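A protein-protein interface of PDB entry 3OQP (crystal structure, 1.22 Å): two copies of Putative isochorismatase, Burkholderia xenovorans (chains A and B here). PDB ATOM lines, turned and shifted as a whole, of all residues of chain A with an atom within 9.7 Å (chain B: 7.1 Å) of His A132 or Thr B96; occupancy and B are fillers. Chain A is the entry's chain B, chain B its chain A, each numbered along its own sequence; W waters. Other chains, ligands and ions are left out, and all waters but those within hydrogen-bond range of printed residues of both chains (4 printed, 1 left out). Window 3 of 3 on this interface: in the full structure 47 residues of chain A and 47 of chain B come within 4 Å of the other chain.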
ATOM      1  N   PHE A  95     -18.627 -26.159  10.234  1.00  0.00           N
ATOM      2  CA  PHE A  95     -18.982 -27.225   9.283  1.00  0.00           C
ATOM      3  C   PHE A  95     -19.475 -28.539   9.899  1.00  0.00           C
ATOM      4  O   PHE A  95     -20.315 -29.232   9.314  1.00  0.00           O
ATOM      5  CB  PHE A  95     -17.771 -27.531   8.388  1.00  0.00           C
ATOM      6  CG  PHE A  95     -17.448 -26.456   7.400  1.00  0.00           C
ATOM      7  CD1 PHE A  95     -18.135 -26.370   6.211  1.00  0.00           C
ATOM      8  CD2 PHE A  95     -16.499 -25.493   7.709  1.00  0.00           C
ATOM      9  CE1 PHE A  95     -17.850 -25.411   5.318  1.00  0.00           C
ATOM     10  CE2 PHE A  95     -16.215 -24.476   6.854  1.00  0.00           C
ATOM     11  CZ  PHE A  95     -16.889 -24.424   5.640  1.00  0.00           C
ATOM     12  N   ALA A 124     -10.709 -20.392  13.763  1.00  0.00           N
ATOM     13  CA  ALA A 124      -9.593 -21.187  13.178  1.00  0.00           C
ATOM     14  C   ALA A 124     -10.052 -22.563  12.743  1.00  0.00           C
ATOM     15  O   ALA A 124      -9.649 -23.030  11.653  1.00  0.00           O
ATOM     16  CB  ALA A 124      -8.442 -21.289  14.184  1.00  0.00           C
ATOM     17  N   SER A 125     -10.879 -23.206  13.560  1.00  0.00           N
ATOM     18  CA  SER A 125     -11.343 -24.536  13.158  1.00  0.00           C
ATOM     19  C   SER A 125     -12.204 -24.526  11.908  1.00  0.00           C
ATOM     20  O   SER A 125     -12.043 -25.394  11.036  1.00  0.00           O
ATOM     21  CB  SER A 125     -12.176 -25.201  14.248  1.00  0.00           C
ATOM     22  OG  SER A 125     -11.400 -25.419  15.395  1.00  0.00           O
ATOM     23  N   THR A 126     -13.081 -23.554  11.795  1.00  0.00           N
ATOM     24  CA  THR A 126     -13.898 -23.367  10.603  1.00  0.00           C
ATOM     25  C   THR A 126     -13.035 -23.116   9.370  1.00  0.00           C
ATOM     26  O   THR A 126     -13.255 -23.709   8.284  1.00  0.00           O
ATOM     27  CB  THR A 126     -14.923 -22.240  10.833  1.00  0.00           C
ATOM     28  OG1 THR A 126     -15.758 -22.548  11.975  1.00  0.00           O
ATOM     29  CG2 THR A 126     -15.765 -21.998   9.581  1.00  0.00           C
ATOM     30  N   ILE A 127     -12.032 -22.258   9.510  1.00  0.00           N
ATOM     31  CA  ILE A 127     -11.121 -21.894   8.428  1.00  0.00           C
ATOM     32  C   ILE A 127     -10.339 -23.116   8.044  1.00  0.00           C
ATOM     33  O   ILE A 127     -10.192 -23.378   6.839  1.00  0.00           O
ATOM     34  CB  ILE A 127     -10.149 -20.806   8.877  1.00  0.00           C
ATOM     35  CG1 ILE A 127     -10.899 -19.487   8.999  1.00  0.00           C
ATOM     36  CG2 ILE A 127      -9.001 -20.665   7.825  1.00  0.00           C
ATOM     37  CD1 ILE A 127     -10.134 -18.327   9.672  1.00  0.00           C
ATOM     38  N   ASN A 128      -9.843 -23.921   8.944  1.00  0.00           N
ATOM     39  CA  ASN A 128      -9.032 -25.082   8.598  1.00  0.00           C
ATOM     40  C   ASN A 128      -9.841 -26.119   7.807  1.00  0.00           C
ATOM     41  O   ASN A 128      -9.393 -26.604   6.745  1.00  0.00           O
ATOM     42  CB  ASN A 128      -8.359 -25.642   9.858  1.00  0.00           C
ATOM     43  CG  ASN A 128      -7.007 -26.244   9.538  1.00  0.00           C
ATOM     44  OD1 ASN A 128      -6.986 -27.220   8.951  1.00  0.00           O
ATOM     45  ND2 ASN A 128      -5.904 -25.590   9.894  1.00  0.00           N
ATOM     46  N   HIS A 129     -11.087 -26.337   8.216  1.00  0.00           N
ATOM     47  CA  HIS A 129     -12.006 -27.178   7.428  1.00  0.00           C
ATOM     48  C   HIS A 129     -12.236 -26.596   6.016  1.00  0.00           C
ATOM     49  O   HIS A 129     -12.188 -27.307   5.016  1.00  0.00           O
ATOM     50  CB  HIS A 129     -13.334 -27.378   8.158  1.00  0.00           C
ATOM     51  CG  HIS A 129     -13.322 -28.504   9.149  1.00  0.00           C
ATOM     52  ND1 HIS A 129     -14.158 -28.518  10.232  1.00  0.00           N
ATOM     53  CD2 HIS A 129     -12.660 -29.689   9.166  1.00  0.00           C
ATOM     54  CE1 HIS A 129     -13.994 -29.655  10.897  1.00  0.00           C
ATOM     55  NE2 HIS A 129     -13.076 -30.382  10.281  1.00  0.00           N
ATOM     56  N   ALA A 130     -12.549 -25.303   5.901  1.00  0.00           N
ATOM     57  CA  ALA A 130     -12.831 -24.684   4.636  1.00  0.00           C
ATOM     58  C   ALA A 130     -11.699 -24.802   3.655  1.00  0.00           C
ATOM     59  O   ALA A 130     -11.922 -25.190   2.519  1.00  0.00           O
ATOM     60  CB  ALA A 130     -13.173 -23.207   4.810  1.00  0.00           C
ATOM     61  N   VAL A 131     -10.496 -24.476   4.107  1.00  0.00           N
ATOM     62  CA  VAL A 131      -9.334 -24.574   3.254  1.00  0.00           C
ATOM     63  C   VAL A 131      -9.148 -25.994   2.731  1.00  0.00           C
ATOM     64  O   VAL A 131      -8.876 -26.226   1.556  1.00  0.00           O
ATOM     65  CB  VAL A 131      -8.036 -24.091   4.031  1.00  0.00           C
ATOM     66  CG1 VAL A 131      -6.747 -24.486   3.250  1.00  0.00           C
ATOM     67  CG2 VAL A 131      -8.114 -22.588   4.221  1.00  0.00           C
ATOM     68  N   HIS A 132      -9.278 -26.979   3.606  1.00  0.00           N
ATOM     69  CA  HIS A 132      -9.071 -28.354   3.203  1.00  0.00           C
ATOM     70  C   HIS A 132     -10.177 -28.913   2.293  1.00  0.00           C
ATOM     71  O   HIS A 132      -9.945 -29.904   1.610  1.00  0.00           O
ATOM     72  CB  HIS A 132      -8.733 -29.261   4.400  1.00  0.00           C
ATOM     73  CG  HIS A 132      -7.372 -29.029   4.954  1.00  0.00           C
ATOM     74  ND1 HIS A 132      -7.091 -28.090   5.922  1.00  0.00           N
ATOM     75  CD2 HIS A 132      -6.196 -29.647   4.681  1.00  0.00           C
ATOM     76  CE1 HIS A 132      -5.802 -28.131   6.198  1.00  0.00           C
ATOM     77  NE2 HIS A 132      -5.225 -29.053   5.444  1.00  0.00           N
ATOM     78  N   SER A 133     -11.337 -28.257   2.262  1.00  0.00           N
ATOM     79  CA  SER A 133     -12.432 -28.595   1.366  1.00  0.00           C
ATOM     80  C   SER A 133     -12.288 -27.912   0.031  1.00  0.00           C
ATOM     81  O   SER A 133     -12.973 -28.323  -0.903  1.00  0.00           O
ATOM     82  CB  SER A 133     -13.772 -28.177   2.022  1.00  0.00           C
ATOM     83  OG  SER A 133     -14.109 -26.804   1.797  1.00  0.00           O
ATOM     84  N   GLY A 134     -11.340 -26.982  -0.097  1.00  0.00           N
ATOM     85  CA  GLY A 134     -11.077 -26.277  -1.356  1.00  0.00           C
ATOM     86  C   GLY A 134     -11.578 -24.868  -1.487  1.00  0.00           C
ATOM     87  O   GLY A 134     -11.496 -24.273  -2.539  1.00  0.00           O
ATOM     88  N   LEU A 135     -12.179 -24.349  -0.436  1.00  0.00           N
ATOM     89  CA  LEU A 135     -12.579 -22.940  -0.401  1.00  0.00           C
ATOM     90  C   LEU A 135     -11.389 -21.998  -0.175  1.00  0.00           C
ATOM     91  O   LEU A 135     -10.465 -22.337   0.561  1.00  0.00           O
ATOM     92  CB  LEU A 135     -13.599 -22.742   0.733  1.00  0.00           C
ATOM     93  CG  LEU A 135     -14.955 -23.408   0.535  1.00  0.00           C
ATOM     94  CD1 LEU A 135     -15.720 -23.376   1.833  1.00  0.00           C
ATOM     95  CD2 LEU A 135     -15.768 -22.751  -0.606  1.00  0.00           C
ATOM     96  N   ALA A 136     -11.468 -20.800  -0.733  1.00  0.00           N
ATOM     97  CA  ALA A 136     -10.612 -19.686  -0.429  1.00  0.00           C
ATOM     98  C   ALA A 136     -11.211 -19.079   0.818  1.00  0.00           C
ATOM     99  O   ALA A 136     -12.453 -19.090   0.973  1.00  0.00           O
ATOM    100  CB  ALA A 136     -10.580 -18.652  -1.477  1.00  0.00           C
ATOM    101  N   VAL A 137     -10.404 -18.544   1.747  1.00  0.00           N
ATOM    102  CA  VAL A 137     -10.864 -18.009   3.018  1.00  0.00           C
ATOM    103  C   VAL A 137     -10.259 -16.637   3.198  1.00  0.00           C
ATOM    104  O   VAL A 137      -9.128 -16.366   2.808  1.00  0.00           O
ATOM    105  CB  VAL A 137     -10.494 -18.945   4.147  1.00  0.00           C
ATOM    106  CG1 VAL A 137     -11.034 -18.392   5.488  1.00  0.00           C
ATOM    107  CG2 VAL A 137     -11.063 -20.328   3.882  1.00  0.00           C
ATOM    108  N   ARG A 172      -0.668 -18.873   5.331  1.00  0.00           N
ATOM    109  CA  ARG A 172      -1.079 -20.094   4.592  1.00  0.00           C
ATOM    110  C   ARG A 172      -2.567 -20.320   4.357  1.00  0.00           C
ATOM    111  O   ARG A 172      -2.931 -20.907   3.324  1.00  0.00           O
ATOM    112  CB  ARG A 172      -0.596 -21.320   5.417  1.00  0.00           C
ATOM    113  CG  ARG A 172      -0.935 -22.694   4.814  1.00  0.00           C
ATOM    114  CD  ARG A 172      -0.370 -22.911   3.495  1.00  0.00           C
ATOM    115  NE  ARG A 172      -0.776 -24.173   2.865  1.00  0.00           N
ATOM    116  CZ  ARG A 172      -1.920 -24.373   2.214  1.00  0.00           C
ATOM    117  NH1 ARG A 172      -2.848 -23.437   2.127  1.00  0.00           N
ATOM    118  NH2 ARG A 172      -2.131 -25.537   1.600  1.00  0.00           N
ATOM    119  N   PHE A 173      -3.389 -19.908   5.319  1.00  0.00           N
ATOM    120  CA  PHE A 173      -4.796 -20.353   5.335  1.00  0.00           C
ATOM    121  C   PHE A 173      -5.810 -19.325   4.849  1.00  0.00           C
ATOM    122  O   PHE A 173      -6.886 -19.738   4.392  1.00  0.00           O
ATOM    123  CB  PHE A 173      -5.178 -20.759   6.773  1.00  0.00           C
ATOM    124  CG  PHE A 173      -4.381 -21.921   7.283  1.00  0.00           C
ATOM    125  CD1 PHE A 173      -4.786 -23.204   7.013  1.00  0.00           C
ATOM    126  CD2 PHE A 173      -3.207 -21.739   7.987  1.00  0.00           C
ATOM    127  CE1 PHE A 173      -4.049 -24.282   7.434  1.00  0.00           C
ATOM    128  CE2 PHE A 173      -2.480 -22.792   8.444  1.00  0.00           C
ATOM    129  CZ  PHE A 173      -2.868 -24.071   8.147  1.00  0.00           C
ATOM    130  N   GLU B  88       2.004 -39.957   2.524  1.00  0.00           N
ATOM    131  CA  GLU B  88       2.492 -38.722   1.916  1.00  0.00           C
ATOM    132  C   GLU B  88       1.350 -37.719   1.775  1.00  0.00           C
ATOM    133  O   GLU B  88       0.228 -38.082   1.499  1.00  0.00           O
ATOM    134  CB  GLU B  88       3.177 -38.944   0.553  1.00  0.00           C
ATOM    135  CG  GLU B  88       2.188 -39.228  -0.591  1.00  0.00           C
ATOM    136  CD  GLU B  88       2.846 -39.184  -1.948  1.00  0.00           C
ATOM    137  OE1 GLU B  88       3.794 -39.955  -2.168  1.00  0.00           O
ATOM    138  OE2 GLU B  88       2.421 -38.358  -2.776  1.00  0.00           O
ATOM    139  N   LYS B  89       1.655 -36.438   1.962  1.00  0.00           N
ATOM    140  CA  LYS B  89       0.676 -35.354   1.842  1.00  0.00           C
ATOM    141  C   LYS B  89       1.308 -34.142   1.135  1.00  0.00           C
ATOM    142  O   LYS B  89       2.531 -34.021   1.063  1.00  0.00           O
ATOM    143  CB  LYS B  89       0.089 -34.937   3.203  1.00  0.00           C
ATOM    144  CG  LYS B  89       1.100 -34.258   4.101  1.00  0.00           C
ATOM    145  CD  LYS B  89       0.498 -33.929   5.463  1.00  0.00           C
ATOM    146  CE  LYS B  89       1.429 -33.117   6.310  1.00  0.00           C
ATOM    147  NZ  LYS B  89       1.652 -31.745   5.805  1.00  0.00           N
ATOM    148  N   SER B  90       0.428 -33.271   0.651  1.00  0.00           N
ATOM    149  CA  SER B  90       0.740 -32.000   0.014  1.00  0.00           C
ATOM    150  C   SER B  90      -0.165 -30.866   0.526  1.00  0.00           C
ATOM    151  O   SER B  90      -0.324 -29.840  -0.141  1.00  0.00           O
ATOM    152  CB  SER B  90       0.583 -32.165  -1.503  1.00  0.00           C
ATOM    153  OG  SER B  90       1.611 -32.973  -1.978  1.00  0.00           O
ATOM    154  N   LEU B  91      -0.865 -31.119   1.630  1.00  0.00           N
ATOM    155  CA  LEU B  91      -1.670 -30.157   2.339  1.00  0.00           C
ATOM    156  C   LEU B  91      -1.253 -30.212   3.808  1.00  0.00           C
ATOM    157  O   LEU B  91      -0.643 -31.183   4.208  1.00  0.00           O
ATOM    158  CB  LEU B  91      -3.179 -30.533   2.277  1.00  0.00           C
ATOM    159  CG  LEU B  91      -3.826 -30.443   0.910  1.00  0.00           C
ATOM    160  CD1 LEU B  91      -5.201 -31.070   0.962  1.00  0.00           C
ATOM    161  CD2 LEU B  91      -3.875 -28.979   0.483  1.00  0.00           C
ATOM    162  N   PRO B  92      -1.607 -29.189   4.608  1.00  0.00           N
ATOM    163  CA  PRO B  92      -1.256 -29.239   6.022  1.00  0.00           C
ATOM    164  C   PRO B  92      -1.755 -30.468   6.776  1.00  0.00           C
ATOM    165  O   PRO B  92      -0.964 -31.158   7.435  1.00  0.00           O
ATOM    166  CB  PRO B  92      -1.818 -27.911   6.571  1.00  0.00           C
ATOM    167  CG  PRO B  92      -1.791 -27.020   5.327  1.00  0.00           C
ATOM    168  CD  PRO B  92      -2.165 -27.891   4.192  1.00  0.00           C
ATOM    169  N   SER B  93      -3.017 -30.829   6.564  1.00  0.00           N
ATOM    170  CA  SER B  93      -3.579 -31.957   7.286  1.00  0.00           C
ATOM    171  C   SER B  93      -3.177 -33.312   6.653  1.00  0.00           C
ATOM    172  O   SER B  93      -3.249 -33.517   5.445  1.00  0.00           O
ATOM    173  CB  SER B  93      -5.089 -31.914   7.264  1.00  0.00           C
ATOM    174  OG  SER B  93      -5.613 -33.118   7.830  1.00  0.00           O
ATOM    175  N   ALA B  94      -2.749 -34.246   7.499  1.00  0.00           N
ATOM    176  CA  ALA B  94      -2.391 -35.600   7.129  1.00  0.00           C
ATOM    177  C   ALA B  94      -3.626 -36.454   6.834  1.00  0.00           C
ATOM    178  O   ALA B  94      -3.479 -37.539   6.267  1.00  0.00           O
ATOM    179  CB  ALA B  94      -1.573 -36.255   8.220  1.00  0.00           C
ATOM    180  N   PHE B  95      -4.833 -35.947   7.087  1.00  0.00           N
ATOM    181  CA  PHE B  95      -6.051 -36.699   6.786  1.00  0.00           C
ATOM    182  C   PHE B  95      -6.627 -36.485   5.407  1.00  0.00           C
ATOM    183  O   PHE B  95      -7.181 -37.416   4.858  1.00  0.00           O
ATOM    184  CB  PHE B  95      -7.141 -36.319   7.804  1.00  0.00           C
ATOM    185  CG  PHE B  95      -6.967 -36.919   9.193  1.00  0.00           C
ATOM    186  CD1 PHE B  95      -7.388 -38.206   9.447  1.00  0.00           C
ATOM    187  CD2 PHE B  95      -6.379 -36.216  10.207  1.00  0.00           C
ATOM    188  CE1 PHE B  95      -7.255 -38.778  10.694  1.00  0.00           C
ATOM    189  CE2 PHE B  95      -6.221 -36.779  11.493  1.00  0.00           C
ATOM    190  CZ  PHE B  95      -6.668 -38.030  11.740  1.00  0.00           C
ATOM    191  N   THR B  96      -6.587 -35.262   4.924  1.00  0.00           N
ATOM    192  CA  THR B  96      -7.357 -34.931   3.715  1.00  0.00           C
ATOM    193  C   THR B  96      -6.956 -35.703   2.487  1.00  0.00           C
ATOM    194  O   THR B  96      -5.869 -35.586   2.000  1.00  0.00           O
ATOM    195  CB  THR B  96      -7.314 -33.435   3.397  1.00  0.00           C
ATOM    196  OG1 THR B  96      -7.687 -32.713   4.574  1.00  0.00           O
ATOM    197  CG2 THR B  96      -8.169 -33.030   2.182  1.00  0.00           C
ATOM    198  N   GLY B  97      -7.881 -36.559   2.089  1.00  0.00           N
ATOM    199  CA  GLY B  97      -7.766 -37.373   0.945  1.00  0.00           C
ATOM    200  C   GLY B  97      -6.889 -38.601   1.109  1.00  0.00           C
ATOM    201  O   GLY B  97      -6.698 -39.303   0.123  1.00  0.00           O
ATOM    202  N   THR B  98      -6.338 -38.838   2.307  1.00  0.00           N
ATOM    203  CA  THR B  98      -5.357 -39.920   2.523  1.00  0.00           C
ATOM    204  C   THR B  98      -6.029 -41.155   3.085  1.00  0.00           C
ATOM    205  O   THR B  98      -7.247 -41.153   3.330  1.00  0.00           O
ATOM    206  CB  THR B  98      -4.231 -39.457   3.463  1.00  0.00           C
ATOM    207  OG1 THR B  98      -4.727 -39.428   4.810  1.00  0.00           O
ATOM    208  CG2 THR B  98      -3.648 -38.051   3.055  1.00  0.00           C
ATOM    209  N   ASP B  99      -5.238 -42.187   3.367  1.00  0.00           N
ATOM    210  CA  ASP B  99      -5.781 -43.374   3.975  1.00  0.00           C
ATOM    211  C   ASP B  99      -5.739 -43.359   5.511  1.00  0.00           C
ATOM    212  O   ASP B  99      -6.037 -44.384   6.122  1.00  0.00           O
ATOM    213  CB  ASP B  99      -5.107 -44.603   3.432  1.00  0.00           C
ATOM    214  CG  ASP B  99      -3.693 -44.786   3.900  1.00  0.00           C
ATOM    215  OD1 ASP B  99      -3.226 -44.064   4.805  1.00  0.00           O
ATOM    216  OD2 ASP B  99      -3.050 -45.741   3.368  1.00  0.00           O
ATOM    217  N   LEU B 100      -5.403 -42.203   6.123  1.00  0.00           N
ATOM    218  CA  LEU B 100      -5.074 -42.172   7.539  1.00  0.00           C
ATOM    219  C   LEU B 100      -6.274 -42.543   8.420  1.00  0.00           C
ATOM    220  O   LEU B 100      -6.152 -43.411   9.264  1.00  0.00           O
ATOM    221  CB  LEU B 100      -4.533 -40.782   7.943  1.00  0.00           C
ATOM    222  CG  LEU B 100      -4.138 -40.605   9.411  1.00  0.00           C
ATOM    223  CD1 LEU B 100      -3.079 -41.666   9.801  1.00  0.00           C
ATOM    224  CD2 LEU B 100      -3.645 -39.206   9.648  1.00  0.00           C
ATOM    225  N   ASN B 121       0.806 -25.513  11.897  1.00  0.00           N
ATOM    226  CA  ASN B 121       0.430 -25.676  10.530  1.00  0.00           C
ATOM    227  C   ASN B 121       0.033 -27.127  10.319  1.00  0.00           C
ATOM    228  O   ASN B 121      -1.155 -27.466  10.446  1.00  0.00           O
ATOM    229  CB  ASN B 121       1.578 -25.189   9.625  1.00  0.00           C
ATOM    230  CG  ASN B 121       1.162 -24.978   8.180  1.00  0.00           C
ATOM    231  OD1 ASN B 121       0.631 -23.954   7.831  1.00  0.00           O
ATOM    232  ND2 ASN B 121       1.429 -25.954   7.311  1.00  0.00           N
ATOM    233  N   SER B 125      -3.475 -28.523  11.909  1.00  0.00           N
ATOM    234  CA  SER B 125      -4.466 -28.925  10.912  1.00  0.00           C
ATOM    235  C   SER B 125      -4.895 -30.364  11.106  1.00  0.00           C
ATOM    236  O   SER B 125      -6.094 -30.699  11.057  1.00  0.00           O
ATOM    237  CB  SER B 125      -3.895 -28.687   9.519  1.00  0.00           C
ATOM    238  OG  SER B 125      -3.753 -27.309   9.227  1.00  0.00           O
ATOM    239  N   THR B 126      -3.918 -31.226  11.316  1.00  0.00           N
ATOM    240  CA  THR B 126      -4.149 -32.627  11.500  1.00  0.00           C
ATOM    241  C   THR B 126      -4.985 -32.848  12.767  1.00  0.00           C
ATOM    242  O   THR B 126      -5.976 -33.640  12.760  1.00  0.00           O
ATOM    243  CB  THR B 126      -2.835 -33.408  11.561  1.00  0.00           C
ATOM    244  OG1 THR B 126      -2.148 -33.248  10.305  1.00  0.00           O
ATOM    245  CG2 THR B 126      -3.023 -34.882  11.817  1.00  0.00           C
ATOM    246  N   ASN B 128      -7.054 -30.656  14.193  1.00  0.00           N
ATOM    247  CA  ASN B 128      -8.391 -30.111  13.997  1.00  0.00           C
ATOM    248  C   ASN B 128      -9.283 -31.151  13.332  1.00  0.00           C
ATOM    249  O   ASN B 128     -10.418 -31.389  13.779  1.00  0.00           O
ATOM    250  CB  ASN B 128      -8.364 -28.849  13.112  1.00  0.00           C
ATOM    251  CG  ASN B 128      -9.769 -28.248  12.905  1.00  0.00           C
ATOM    252  OD1 ASN B 128     -10.363 -27.945  13.887  1.00  0.00           O
ATOM    253  ND2 ASN B 128     -10.298 -28.115  11.639  1.00  0.00           N
ATOM    254  N   HIS B 129      -8.764 -31.826  12.307  1.00  0.00           N
ATOM    255  CA  HIS B 129      -9.513 -32.872  11.637  1.00  0.00           C
ATOM    256  C   HIS B 129      -9.791 -34.019  12.610  1.00  0.00           C
ATOM    257  O   HIS B 129     -10.912 -34.535  12.685  1.00  0.00           O
ATOM    258  CB  HIS B 129      -8.778 -33.353  10.390  1.00  0.00           C
ATOM    259  CG  HIS B 129      -9.026 -32.503   9.190  1.00  0.00           C
ATOM    260  ND1 HIS B 129      -8.057 -32.265   8.235  1.00  0.00           N
ATOM    261  CD2 HIS B 129     -10.160 -31.928   8.726  1.00  0.00           C
ATOM    262  CE1 HIS B 129      -8.578 -31.527   7.274  1.00  0.00           C
ATOM    263  NE2 HIS B 129      -9.853 -31.320   7.531  1.00  0.00           N
HETATM  264  O   HOH W   1     -11.783 -30.212   5.561  1.00  0.00           O
HETATM  265  O   HOH W   2       0.106 -27.152   0.957  1.00  0.00           O
HETATM  266  O   HOH W   3     -12.777 -33.241  10.754  1.00  0.00           O
HETATM  267  O   HOH W   4      -8.636 -28.947   9.659  1.00  0.00           O
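Ser A125 touches Asn B128, and with the chains exchanged Asn A128 touches Ser B125. Asn B128 touches its own counterpart, Asn A128. His A129 touches Asn B128, but with the chains exchanged Asn A128 does not touch His B129 (4.8 Å). His A129 touches its own counterpart, His B129. Positions printed for both chains: 95, 125, 126, 128 and 129. Of the 15 pairs that touch across the chains among the printed residues, 4 have their exchanged pair printed and touching as well.
Among the printed residues, pairs that only touch across the chains: Phe A173 with Asn B121 (3.4 Å), His A129 with His B129 (3.4 Å), His A132 with Thr B96 (3.4 Å), Arg A172 with Pro B92 (3.5 Å), His A132 with Pro B92 (3.5 Å), Phe A173 with Ser B125 (3.5 Å), Asn A128 with Asn B128 (3.6 Å), His A132 with His B129 (3.6 Å), Arg A172 with Asn B121 (3.6 Å), His A132 with Ser B125 (3.7 Å), His A129 with Asn B128 (3.8 Å) and His A132 with Leu B91 (3.96 Å).
Of the printed residues of chain B, His A132 touches Leu B91, Pro B92, Ser B93, Thr B96, Ser B125 and His B129. Of chain A, only His A132 (3.4 Å) comes within 4 Å of Thr B96. Pro B92 touches just these residues of chain A: His A132 and Arg A172. Ser B93 touches one residue of chain A. No residue of chain A comes within 4 Å of Gly B97. No residue of chain A comes within 4 Å of Thr B98. Printed residues of chain B within 4 Å of His A129: Asn B128 (3.8 Å) and His B129 (3.4 Å). Printed residues of chain A within 4 Å of Ser B125: Asn A128 (2.8 Å), His A132 (3.7 Å) and Phe A173 (3.5 Å). Of the printed residues of chain B, Ser A125 touches Asn B128. Of the printed residues of chain B, Asn A128 touches Ser B125 (2.8 Å) and Asn B128 (3.6 Å). Of the printed residues of chain A, His B129 touches His A129 and His A132. Ala A124 touches none of the printed residues of chain B. Val A137 touches none of the printed residues of chain B. The nearest printed residue of chain A that does not touch Asn B121 is Asn A128 (5.1 Å).
Water W4 lies within hydrogen-bond range of the side-chain amide oxygen (OD1) of Asn A128 (2.5 Å), the side-chain amide nitrogen (ND2) of Asn B128 (2.7 Å), the backbone carbonyl oxygen (O) of Ser B125 (3.4 Å) and a ring nitrogen (NE2) of His B129 (3.4 Å). Water W2 bridges NH2 of Arg A172 and O of Ser B90. Water W3 lies within hydrogen-bond range of NE2 of His A129 (2.9 Å) and O of His B129 (3.0 Å). Water W1 lies within hydrogen-bond range of NE2 of His B129 (3.0 Å) and O of His A129 (3.0 Å).
A ring nitrogen (NE2) of His A132 lies within hydrogen-bond range of the backbone NH (N) of Ser B93, 3.0 Å away. OG of Ser B125 is in hydrogen-bond range of ND2 of Asn A128, at 2.8 Å. The side-chain amide oxygen of Asn B128 sits at hydrogen-bond distance from the side-chain hydroxyl of Ser A125, 3.1 Å away.
Hydrophobic or aromatic side chains of chain B that line the printed part of chain A: Leu B91, Pro B92 and His B129. Along chain B the printed residues that touch a printed residue of chain A span positions 91 to 129. Printed residues of chain A that touch a printed residue of chain B: Ser A125, Asn A128, His A129, His A132, Arg A172 and Phe A173. Among the printed residues, 15 pairs touch across the chains. Among the printed residues, no Asp or Glu carboxylate lies within 4 Å of a Lys or Arg side-chain nitrogen of the other chain.
The side-chain amino group (NZ) of Lys B89 is in hydrogen-bond range of the backbone carbonyl oxygen (O) of Leu B91. O of Pro B92 lies within hydrogen-bond range of NZ of Lys B89 (3.1 Å). N of Phe B95 sits at hydrogen-bond distance from OG of Ser B93 (3.0 Å). The side-chain hydroxyl (OG) of Ser B93 lies within hydrogen-bond range of a ring nitrogen (ND1) of His B129. The side-chain hydroxyl (OG) of Ser B125 sits at hydrogen-bond distance from the backbone carbonyl oxygen (O) of Asn B121 (2.9 Å). ND1 of His A132 lies within hydrogen-bond range of O of Asn A128 (2.9 Å).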
